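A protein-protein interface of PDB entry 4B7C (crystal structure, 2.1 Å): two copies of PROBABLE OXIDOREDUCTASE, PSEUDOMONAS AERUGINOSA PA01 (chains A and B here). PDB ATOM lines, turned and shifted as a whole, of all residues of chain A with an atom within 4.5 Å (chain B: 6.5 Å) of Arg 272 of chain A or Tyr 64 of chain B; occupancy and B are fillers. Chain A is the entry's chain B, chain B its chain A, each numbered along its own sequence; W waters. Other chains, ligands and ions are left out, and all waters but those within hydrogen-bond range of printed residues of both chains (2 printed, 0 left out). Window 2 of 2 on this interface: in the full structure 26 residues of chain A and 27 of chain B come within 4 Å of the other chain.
N of Gly 277 of chain B is in hydrogen-bond range of O of Ala 273 of chain A (3.1 Å). OD2 of Asp 282 of chain B is in salt-bridge range of NE of Arg 272 of chain A, 2.8 Å away.
O of Leu 268 of chain A touches CA of Gly 277 of chain B (3.4 Å). O of Cys 247 of chain B touches CD2 of Leu 269 of chain A (3.9 Å). Gln 252 of chain B touches Leu 269 of chain A. Leu 269 of chain A touches Gly 277 of chain B. CD1 of Leu 269 of chain A touches O of Met 278 of chain B, at 2.9 Å. CG1 of Val 270 of chain A touches NH2 of Arg 62 of chain B (3.8 Å). Asn 271 of chain A touches Arg 62 of chain B. Tyr 64 of chain B touches Arg 272 of chain A. CA of Arg 272 of chain A touches O of Gly 277 of chain B (3.5 Å). Arg 272 of chain A touches Met 278 of chain B.
Arg 272 of chain A touches five residues of chain B. Of chain A, only Arg 272 comes within 4 Å of Tyr 64 of chain B. Printed residues of chain A within 4 Å of Met 278 of chain B: Leu 269 (2.9 Å) and Arg 272 (3.9 Å). Printed residues of chain B within 4 Å of Ala 273 of chain A: Glu 276 and Gly 277. Of the printed residues of chain A, Val 279 of chain B touches Arg 272 (3.8 Å). Of the printed residues of chain B, Val 270 of chain A touches Arg 62 (3.8 Å). Ser 267 of chain A touches none of the printed residues of chain B. Ile 65 of chain B touches none of the printed residues of chain A. The nearest residue of chain B that does not touch Arg 272 of chain A is Glu 276 of chain B (5.0 Å). The nearest residue of chain A that does not touch Tyr 64 of chain B is Val 270 of chain A (4.2 Å).
No position is printed for both chains.
The side-chain amide nitrogen (NE2) of Gln 252 of chain B lies within hydrogen-bond range of the side-chain hydroxyl (OH) of Tyr 253 of chain B, 3.2 Å away. The backbone NH of Lys 241 of chain A sits at hydrogen-bond distance from the backbone carbonyl oxygen of Asn 271 of chain A. ND2 of Asn 271 of chain A sits at hydrogen-bond distance from OG of Ser 267 of chain A, at 2.8 Å. The backbone carbonyl oxygen of Leu 268 of chain A sits at hydrogen-bond distance from the backbone NH of Ala 273 of chain A. The guanidinium group of Arg 272 of chain A sits at hydrogen-bond distance from the backbone carbonyl oxygen of Val 270 of chain A (3.0 Å).
Of the 17 printed residues of chain B, 9 touch a printed residue of chain A. Printed residues of chain B that touch a printed residue of chain A: Arg 62, Tyr 64, Cys 247, Gln 252, Glu 276, Gly 277, Met 278, Val 279 and Asp 282. Of the 9 printed residues of chain A, 6 touch a printed residue of chain B. Hydrophobic or aromatic side chains of chain A within 4 Å of the printed part of chain B: Leu 269 and Val 270.
Water W1 bridges the backbone carbonyl oxygen (O) of Arg 272 of chain A (2.8 Å) and the side-chain carboxylate (OE2) of Glu 276 of chain B (3.0 Å). Water W2 bridges NH1 of Arg 272 of chain A and O of Tyr 64 of chain B.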
ATOM      1  N   PHE A 240      -0.491   5.604 -21.149  1.00  0.00           N
ATOM      2  CA  PHE A 240      -1.870   6.014 -21.357  1.00  0.00           C
ATOM      3  C   PHE A 240      -2.049   6.570 -22.781  1.00  0.00           C
ATOM      4  O   PHE A 240      -1.281   7.423 -23.220  1.00  0.00           O
ATOM      5  CB  PHE A 240      -2.247   7.067 -20.300  1.00  0.00           C
ATOM      6  CG  PHE A 240      -3.621   7.654 -20.468  1.00  0.00           C
ATOM      7  CD1 PHE A 240      -4.760   6.855 -20.367  1.00  0.00           C
ATOM      8  CD2 PHE A 240      -3.782   9.018 -20.684  1.00  0.00           C
ATOM      9  CE1 PHE A 240      -6.024   7.403 -20.505  1.00  0.00           C
ATOM     10  CE2 PHE A 240      -5.046   9.572 -20.824  1.00  0.00           C
ATOM     11  CZ  PHE A 240      -6.171   8.765 -20.731  1.00  0.00           C
ATOM     12  N   LYS A 241      -3.064   6.061 -23.483  1.00  0.00           N
ATOM     13  CA  LYS A 241      -3.405   6.487 -24.861  1.00  0.00           C
ATOM     14  C   LYS A 241      -2.299   6.179 -25.887  1.00  0.00           C
ATOM     15  O   LYS A 241      -2.166   6.856 -26.908  1.00  0.00           O
ATOM     16  CB  LYS A 241      -3.807   7.976 -24.919  1.00  0.00           C
ATOM     17  CG  LYS A 241      -5.187   8.230 -24.305  1.00  0.00           C
ATOM     18  CD  LYS A 241      -5.831   9.585 -24.386  1.00  0.00           C
ATOM     19  CE  LYS A 241      -7.360   9.536 -24.439  1.00  0.00           C
ATOM     20  NZ  LYS A 241      -7.972   9.007 -25.690  1.00  0.00           N
ATOM     21  N   SER A 267      -3.240  -4.844 -21.537  1.00  0.00           N
ATOM     22  CA  SER A 267      -2.594  -3.549 -21.304  1.00  0.00           C
ATOM     23  C   SER A 267      -3.277  -2.453 -22.126  1.00  0.00           C
ATOM     24  O   SER A 267      -3.299  -1.288 -21.736  1.00  0.00           O
ATOM     25  CB  SER A 267      -1.097  -3.617 -21.642  1.00  0.00           C
ATOM     26  OG  SER A 267      -0.483  -2.378 -21.345  1.00  0.00           O
ATOM     27  N   LEU A 268      -3.820  -2.831 -23.275  1.00  0.00           N
ATOM     28  CA  LEU A 268      -4.609  -1.894 -24.122  1.00  0.00           C
ATOM     29  C   LEU A 268      -5.855  -1.375 -23.427  1.00  0.00           C
ATOM     30  O   LEU A 268      -6.259  -0.224 -23.621  1.00  0.00           O
ATOM     31  CB  LEU A 268      -5.022  -2.563 -25.430  1.00  0.00           C
ATOM     32  CG  LEU A 268      -3.911  -2.978 -26.392  1.00  0.00           C
ATOM     33  CD1 LEU A 268      -4.475  -3.807 -27.536  1.00  0.00           C
ATOM     34  CD2 LEU A 268      -3.148  -1.761 -26.893  1.00  0.00           C
ATOM     35  N   LEU A 269      -6.439  -2.216 -22.584  1.00  0.00           N
ATOM     36  CA  LEU A 269      -7.556  -1.807 -21.717  1.00  0.00           C
ATOM     37  C   LEU A 269      -7.076  -0.906 -20.571  1.00  0.00           C
ATOM     38  O   LEU A 269      -7.562   0.210 -20.388  1.00  0.00           O
ATOM     39  CB  LEU A 269      -8.274  -3.047 -21.161  1.00  0.00           C
ATOM     40  CG  LEU A 269      -9.403  -2.829 -20.140  1.00  0.00           C
ATOM     41  CD1 LEU A 269     -10.464  -1.882 -20.651  1.00  0.00           C
ATOM     42  CD2 LEU A 269     -10.040  -4.166 -19.808  1.00  0.00           C
ATOM     43  N   VAL A 270      -6.125  -1.413 -19.791  1.00  0.00           N
ATOM     44  CA  VAL A 270      -5.580  -0.680 -18.631  1.00  0.00           C
ATOM     45  C   VAL A 270      -5.108   0.724 -19.003  1.00  0.00           C
ATOM     46  O   VAL A 270      -5.391   1.708 -18.313  1.00  0.00           O
ATOM     47  CB  VAL A 270      -4.417  -1.471 -18.007  1.00  0.00           C
ATOM     48  CG1 VAL A 270      -3.824  -0.706 -16.832  1.00  0.00           C
ATOM     49  CG2 VAL A 270      -4.907  -2.839 -17.566  1.00  0.00           C
ATOM     50  N   ASN A 271      -4.436   0.815 -20.147  1.00  0.00           N
ATOM     51  CA  ASN A 271      -3.904   2.083 -20.655  1.00  0.00           C
ATOM     52  C   ASN A 271      -4.778   2.787 -21.701  1.00  0.00           C
ATOM     53  O   ASN A 271      -4.414   3.843 -22.230  1.00  0.00           O
ATOM     54  CB  ASN A 271      -2.509   1.827 -21.218  1.00  0.00           C
ATOM     55  CG  ASN A 271      -1.539   1.403 -20.139  1.00  0.00           C
ATOM     56  OD1 ASN A 271      -1.233   2.193 -19.255  1.00  0.00           O
ATOM     57  ND2 ASN A 271      -1.092   0.150 -20.180  1.00  0.00           N
ATOM     58  N   ARG A 272      -5.940   2.207 -21.972  1.00  0.00           N
ATOM     59  CA  ARG A 272      -6.900   2.771 -22.944  1.00  0.00           C
ATOM     60  C   ARG A 272      -6.167   3.183 -24.226  1.00  0.00           C
ATOM     61  O   ARG A 272      -6.237   4.313 -24.703  1.00  0.00           O
ATOM     62  CB  ARG A 272      -7.686   3.919 -22.333  1.00  0.00           C
ATOM     63  CG  ARG A 272      -8.570   3.452 -21.193  1.00  0.00           C
ATOM     64  CD  ARG A 272      -7.841   3.498 -19.850  1.00  0.00           C
ATOM     65  NE  ARG A 272      -8.018   4.781 -19.182  1.00  0.00           N
ATOM     66  CZ  ARG A 272      -7.451   5.117 -18.023  1.00  0.00           C
ATOM     67  NH1 ARG A 272      -6.644   4.268 -17.397  1.00  0.00           N
ATOM     68  NH2 ARG A 272      -7.694   6.306 -17.497  1.00  0.00           N
ATOM     69  N   ALA A 273      -5.461   2.200 -24.744  1.00  0.00           N
ATOM     70  CA  ALA A 273      -4.556   2.342 -25.863  1.00  0.00           C
ATOM     71  C   ALA A 273      -5.129   1.658 -27.090  1.00  0.00           C
ATOM     72  O   ALA A 273      -6.075   0.878 -26.995  1.00  0.00           O
ATOM     73  CB  ALA A 273      -3.225   1.685 -25.516  1.00  0.00           C
ATOM     74  N   ALA B  53     -16.259  -6.806 -11.884  1.00  0.00           N
ATOM     75  CA  ALA B  53     -15.099  -5.965 -11.614  1.00  0.00           C
ATOM     76  C   ALA B  53     -14.679  -5.989 -10.137  1.00  0.00           C
ATOM     77  O   ALA B  53     -13.543  -5.672  -9.826  1.00  0.00           O
ATOM     78  CB  ALA B  53     -15.365  -4.537 -12.054  1.00  0.00           C
ATOM     79  N   TRP B  57     -11.009  -5.595  -8.029  1.00  0.00           N
ATOM     80  CA  TRP B  57     -10.819  -4.643  -6.941  1.00  0.00           C
ATOM     81  C   TRP B  57     -10.249  -5.293  -5.723  1.00  0.00           C
ATOM     82  O   TRP B  57      -9.644  -4.617  -4.900  1.00  0.00           O
ATOM     83  CB  TRP B  57     -12.121  -3.938  -6.555  1.00  0.00           C
ATOM     84  CG  TRP B  57     -12.804  -3.233  -7.678  1.00  0.00           C
ATOM     85  CD1 TRP B  57     -12.237  -2.793  -8.874  1.00  0.00           C
ATOM     86  CD2 TRP B  57     -14.215  -2.802  -7.732  1.00  0.00           C
ATOM     87  NE1 TRP B  57     -13.178  -2.156  -9.637  1.00  0.00           N
ATOM     88  CE2 TRP B  57     -14.380  -2.129  -9.017  1.00  0.00           C
ATOM     89  CE3 TRP B  57     -15.317  -2.907  -6.876  1.00  0.00           C
ATOM     90  CZ2 TRP B  57     -15.600  -1.598  -9.419  1.00  0.00           C
ATOM     91  CZ3 TRP B  57     -16.545  -2.373  -7.295  1.00  0.00           C
ATOM     92  CH2 TRP B  57     -16.681  -1.733  -8.538  1.00  0.00           C
ATOM     93  N   ARG B  62      -1.746  -4.279 -10.546  1.00  0.00           N
ATOM     94  CA  ARG B  62      -1.863  -2.936 -11.099  1.00  0.00           C
ATOM     95  C   ARG B  62      -3.023  -2.879 -12.085  1.00  0.00           C
ATOM     96  O   ARG B  62      -3.177  -3.759 -12.929  1.00  0.00           O
ATOM     97  CB  ARG B  62      -0.548  -2.505 -11.763  1.00  0.00           C
ATOM     98  CG  ARG B  62      -0.296  -1.006 -11.877  1.00  0.00           C
ATOM     99  CD  ARG B  62       0.859  -0.620 -12.813  1.00  0.00           C
ATOM    100  NE  ARG B  62       0.457   0.092 -14.038  1.00  0.00           N
ATOM    101  CZ  ARG B  62       0.065  -0.442 -15.204  1.00  0.00           C
ATOM    102  NH1 ARG B  62      -0.042  -1.756 -15.380  1.00  0.00           N
ATOM    103  NH2 ARG B  62      -0.243   0.369 -16.219  1.00  0.00           N
ATOM    104  N   SER B  63      -3.860  -1.858 -11.929  1.00  0.00           N
ATOM    105  CA  SER B  63      -5.015  -1.647 -12.779  1.00  0.00           C
ATOM    106  C   SER B  63      -5.285  -0.152 -12.911  1.00  0.00           C
ATOM    107  O   SER B  63      -4.514   0.681 -12.430  1.00  0.00           O
ATOM    108  CB  SER B  63      -6.244  -2.355 -12.187  1.00  0.00           C
ATOM    109  OG  SER B  63      -7.248  -2.508 -13.181  1.00  0.00           O
ATOM    110  N   TYR B  64      -6.401   0.190 -13.541  1.00  0.00           N
ATOM    111  CA  TYR B  64      -6.794   1.595 -13.689  1.00  0.00           C
ATOM    112  C   TYR B  64      -7.410   2.151 -12.393  1.00  0.00           C
ATOM    113  O   TYR B  64      -7.427   3.363 -12.197  1.00  0.00           O
ATOM    114  CB  TYR B  64      -7.735   1.796 -14.886  1.00  0.00           C
ATOM    115  CG  TYR B  64      -9.021   1.002 -14.858  1.00  0.00           C
ATOM    116  CD1 TYR B  64      -9.083  -0.284 -15.394  1.00  0.00           C
ATOM    117  CD2 TYR B  64     -10.185   1.549 -14.324  1.00  0.00           C
ATOM    118  CE1 TYR B  64     -10.259  -1.015 -15.382  1.00  0.00           C
ATOM    119  CE2 TYR B  64     -11.367   0.827 -14.306  1.00  0.00           C
ATOM    120  CZ  TYR B  64     -11.401  -0.453 -14.838  1.00  0.00           C
ATOM    121  OH  TYR B  64     -12.579  -1.167 -14.829  1.00  0.00           O
ATOM    122  N   ILE B  65      -7.909   1.257 -11.532  1.00  0.00           N
ATOM    123  CA  ILE B  65      -8.362   1.588 -10.163  1.00  0.00           C
ATOM    124  C   ILE B  65      -7.507   0.884  -9.110  1.00  0.00           C
ATOM    125  O   ILE B  65      -7.312  -0.324  -9.201  1.00  0.00           O
ATOM    126  CB  ILE B  65      -9.798   1.088  -9.840  1.00  0.00           C
ATOM    127  CG1 ILE B  65     -10.817   1.542 -10.874  1.00  0.00           C
ATOM    128  CG2 ILE B  65     -10.254   1.632  -8.491  1.00  0.00           C
ATOM    129  CD1 ILE B  65     -12.156   0.837 -10.776  1.00  0.00           C
ATOM    130  N   PRO B  66      -7.084   1.606  -8.054  1.00  0.00           N
ATOM    131  CA  PRO B  66      -6.361   0.929  -6.968  1.00  0.00           C
ATOM    132  C   PRO B  66      -7.147  -0.208  -6.280  1.00  0.00           C
ATOM    133  O   PRO B  66      -8.370  -0.128  -6.130  1.00  0.00           O
ATOM    134  CB  PRO B  66      -6.084   2.059  -5.962  1.00  0.00           C
ATOM    135  CG  PRO B  66      -6.233   3.322  -6.740  1.00  0.00           C
ATOM    136  CD  PRO B  66      -7.296   3.032  -7.755  1.00  0.00           C
ATOM    137  N   CYS B 247     -13.568  -3.962 -23.433  1.00  0.00           N
ATOM    138  CA  CYS B 247     -14.154  -3.433 -22.189  1.00  0.00           C
ATOM    139  C   CYS B 247     -13.826  -4.281 -20.967  1.00  0.00           C
ATOM    140  O   CYS B 247     -13.933  -3.817 -19.836  1.00  0.00           O
ATOM    141  CB  CYS B 247     -15.674  -3.346 -22.316  1.00  0.00           C
ATOM    142  SG  CYS B 247     -16.177  -2.098 -23.498  1.00  0.00           S
ATOM    143  N   GLN B 252      -9.330 -11.617 -16.758  1.00  0.00           N
ATOM    144  CA  GLN B 252      -8.723 -10.350 -16.382  1.00  0.00           C
ATOM    145  C   GLN B 252      -8.507 -10.212 -14.909  1.00  0.00           C
ATOM    146  O   GLN B 252      -7.703  -9.396 -14.522  1.00  0.00           O
ATOM    147  CB  GLN B 252      -9.700  -9.248 -16.744  1.00  0.00           C
ATOM    148  CG  GLN B 252      -9.314  -7.808 -16.447  1.00  0.00           C
ATOM    149  CD  GLN B 252     -10.500  -6.880 -16.628  1.00  0.00           C
ATOM    150  OE1 GLN B 252     -11.528  -7.290 -17.175  1.00  0.00           O
ATOM    151  NE2 GLN B 252     -10.360  -5.625 -16.203  1.00  0.00           N
ATOM    152  N   TYR B 253      -9.288 -10.947 -14.119  1.00  0.00           N
ATOM    153  CA  TYR B 253      -9.356 -10.838 -12.678  1.00  0.00           C
ATOM    154  C   TYR B 253      -8.873 -12.153 -12.051  1.00  0.00           C
ATOM    155  O   TYR B 253      -9.630 -12.801 -11.323  1.00  0.00           O
ATOM    156  CB  TYR B 253     -10.817 -10.570 -12.260  1.00  0.00           C
ATOM    157  CG  TYR B 253     -11.447  -9.355 -12.899  1.00  0.00           C
ATOM    158  CD1 TYR B 253     -10.848  -8.116 -12.764  1.00  0.00           C
ATOM    159  CD2 TYR B 253     -12.660  -9.431 -13.609  1.00  0.00           C
ATOM    160  CE1 TYR B 253     -11.404  -6.979 -13.318  1.00  0.00           C
ATOM    161  CE2 TYR B 253     -13.223  -8.293 -14.174  1.00  0.00           C
ATOM    162  CZ  TYR B 253     -12.590  -7.072 -14.027  1.00  0.00           C
ATOM    163  OH  TYR B 253     -13.145  -5.944 -14.588  1.00  0.00           O
ATOM    164  N   GLU B 276      -8.947  -1.505 -29.586  1.00  0.00           N
ATOM    165  CA  GLU B 276      -8.803  -0.397 -28.654  1.00  0.00           C
ATOM    166  C   GLU B 276      -9.519  -0.627 -27.325  1.00  0.00           C
ATOM    167  O   GLU B 276     -10.670  -1.074 -27.274  1.00  0.00           O
ATOM    168  CB  GLU B 276      -9.302   0.900 -29.286  1.00  0.00           C
ATOM    169  CG  GLU B 276      -9.039   2.136 -28.444  1.00  0.00           C
ATOM    170  CD  GLU B 276      -9.316   3.434 -29.178  1.00  0.00           C
ATOM    171  OE1 GLU B 276      -9.434   3.429 -30.416  1.00  0.00           O
ATOM    172  OE2 GLU B 276      -9.419   4.477 -28.511  1.00  0.00           O
ATOM    173  N   GLY B 277      -8.827  -0.289 -26.241  1.00  0.00           N
ATOM    174  CA  GLY B 277      -9.388  -0.406 -24.898  1.00  0.00           C
ATOM    175  C   GLY B 277     -10.054   0.860 -24.437  1.00  0.00           C
ATOM    176  O   GLY B 277      -9.740   1.962 -24.906  1.00  0.00           O
ATOM    177  N   MET B 278     -11.027   0.703 -23.547  1.00  0.00           N
ATOM    178  CA  MET B 278     -11.692   1.845 -22.926  1.00  0.00           C
ATOM    179  C   MET B 278     -12.077   1.539 -21.491  1.00  0.00           C
ATOM    180  O   MET B 278     -12.246   0.391 -21.106  1.00  0.00           O
ATOM    181  CB  MET B 278     -12.942   2.294 -23.717  1.00  0.00           C
ATOM    182  CG  MET B 278     -14.154   1.373 -23.607  1.00  0.00           C
ATOM    183  SD  MET B 278     -15.104   1.483 -22.089  1.00  0.00           S
ATOM    184  CE  MET B 278     -15.911   3.059 -22.237  1.00  0.00           C
ATOM    185  N   VAL B 279     -12.286   2.612 -20.741  1.00  0.00           N
ATOM    186  CA  VAL B 279     -12.747   2.546 -19.366  1.00  0.00           C
ATOM    187  C   VAL B 279     -13.801   3.626 -19.185  1.00  0.00           C
ATOM    188  O   VAL B 279     -13.585   4.772 -19.573  1.00  0.00           O
ATOM    189  CB  VAL B 279     -11.531   2.751 -18.411  1.00  0.00           C
ATOM    190  CG1 VAL B 279     -11.946   3.387 -17.101  1.00  0.00           C
ATOM    191  CG2 VAL B 279     -10.843   1.418 -18.196  1.00  0.00           C
ATOM    192  N   VAL B 280     -14.948   3.267 -18.602  1.00  0.00           N
ATOM    193  CA  VAL B 280     -16.102   4.168 -18.582  1.00  0.00           C
ATOM    194  C   VAL B 280     -15.833   5.453 -17.819  1.00  0.00           C
ATOM    195  O   VAL B 280     -16.356   6.507 -18.177  1.00  0.00           O
ATOM    196  CB  VAL B 280     -17.379   3.471 -18.009  1.00  0.00           C
ATOM    197  CG1 VAL B 280     -17.185   3.031 -16.551  1.00  0.00           C
ATOM    198  CG2 VAL B 280     -18.586   4.383 -18.170  1.00  0.00           C
ATOM    199  N   MET B 281     -15.012   5.383 -16.773  1.00  0.00           N
ATOM    200  CA  MET B 281     -14.747   6.585 -15.955  1.00  0.00           C
ATOM    201  C   MET B 281     -14.042   7.701 -16.738  1.00  0.00           C
ATOM    202  O   MET B 281     -14.168   8.869 -16.386  1.00  0.00           O
ATOM    203  CB  MET B 281     -14.002   6.249 -14.650  1.00  0.00           C
ATOM    204  CG  MET B 281     -14.895   5.675 -13.549  1.00  0.00           C
ATOM    205  SD  MET B 281     -16.423   6.598 -13.226  1.00  0.00           S
ATOM    206  CE  MET B 281     -15.870   7.839 -12.056  1.00  0.00           C
ATOM    207  N   ASP B 282     -13.362   7.356 -17.831  1.00  0.00           N
ATOM    208  CA  ASP B 282     -12.794   8.377 -18.742  1.00  0.00           C
ATOM    209  C   ASP B 282     -13.859   9.265 -19.373  1.00  0.00           C
ATOM    210  O   ASP B 282     -13.558  10.366 -19.844  1.00  0.00           O
ATOM    211  CB  ASP B 282     -11.973   7.742 -19.871  1.00  0.00           C
ATOM    212  CG  ASP B 282     -10.684   7.123 -19.384  1.00  0.00           C
ATOM    213  OD1 ASP B 282     -10.319   7.330 -18.210  1.00  0.00           O
ATOM    214  OD2 ASP B 282     -10.033   6.398 -20.159  1.00  0.00           O
HETATM  215  O   HOH W   1      -6.678   4.682 -27.435  1.00  0.00           O
HETATM  216  O   HOH W   2      -5.936   5.147 -14.626  1.00  0.00           O
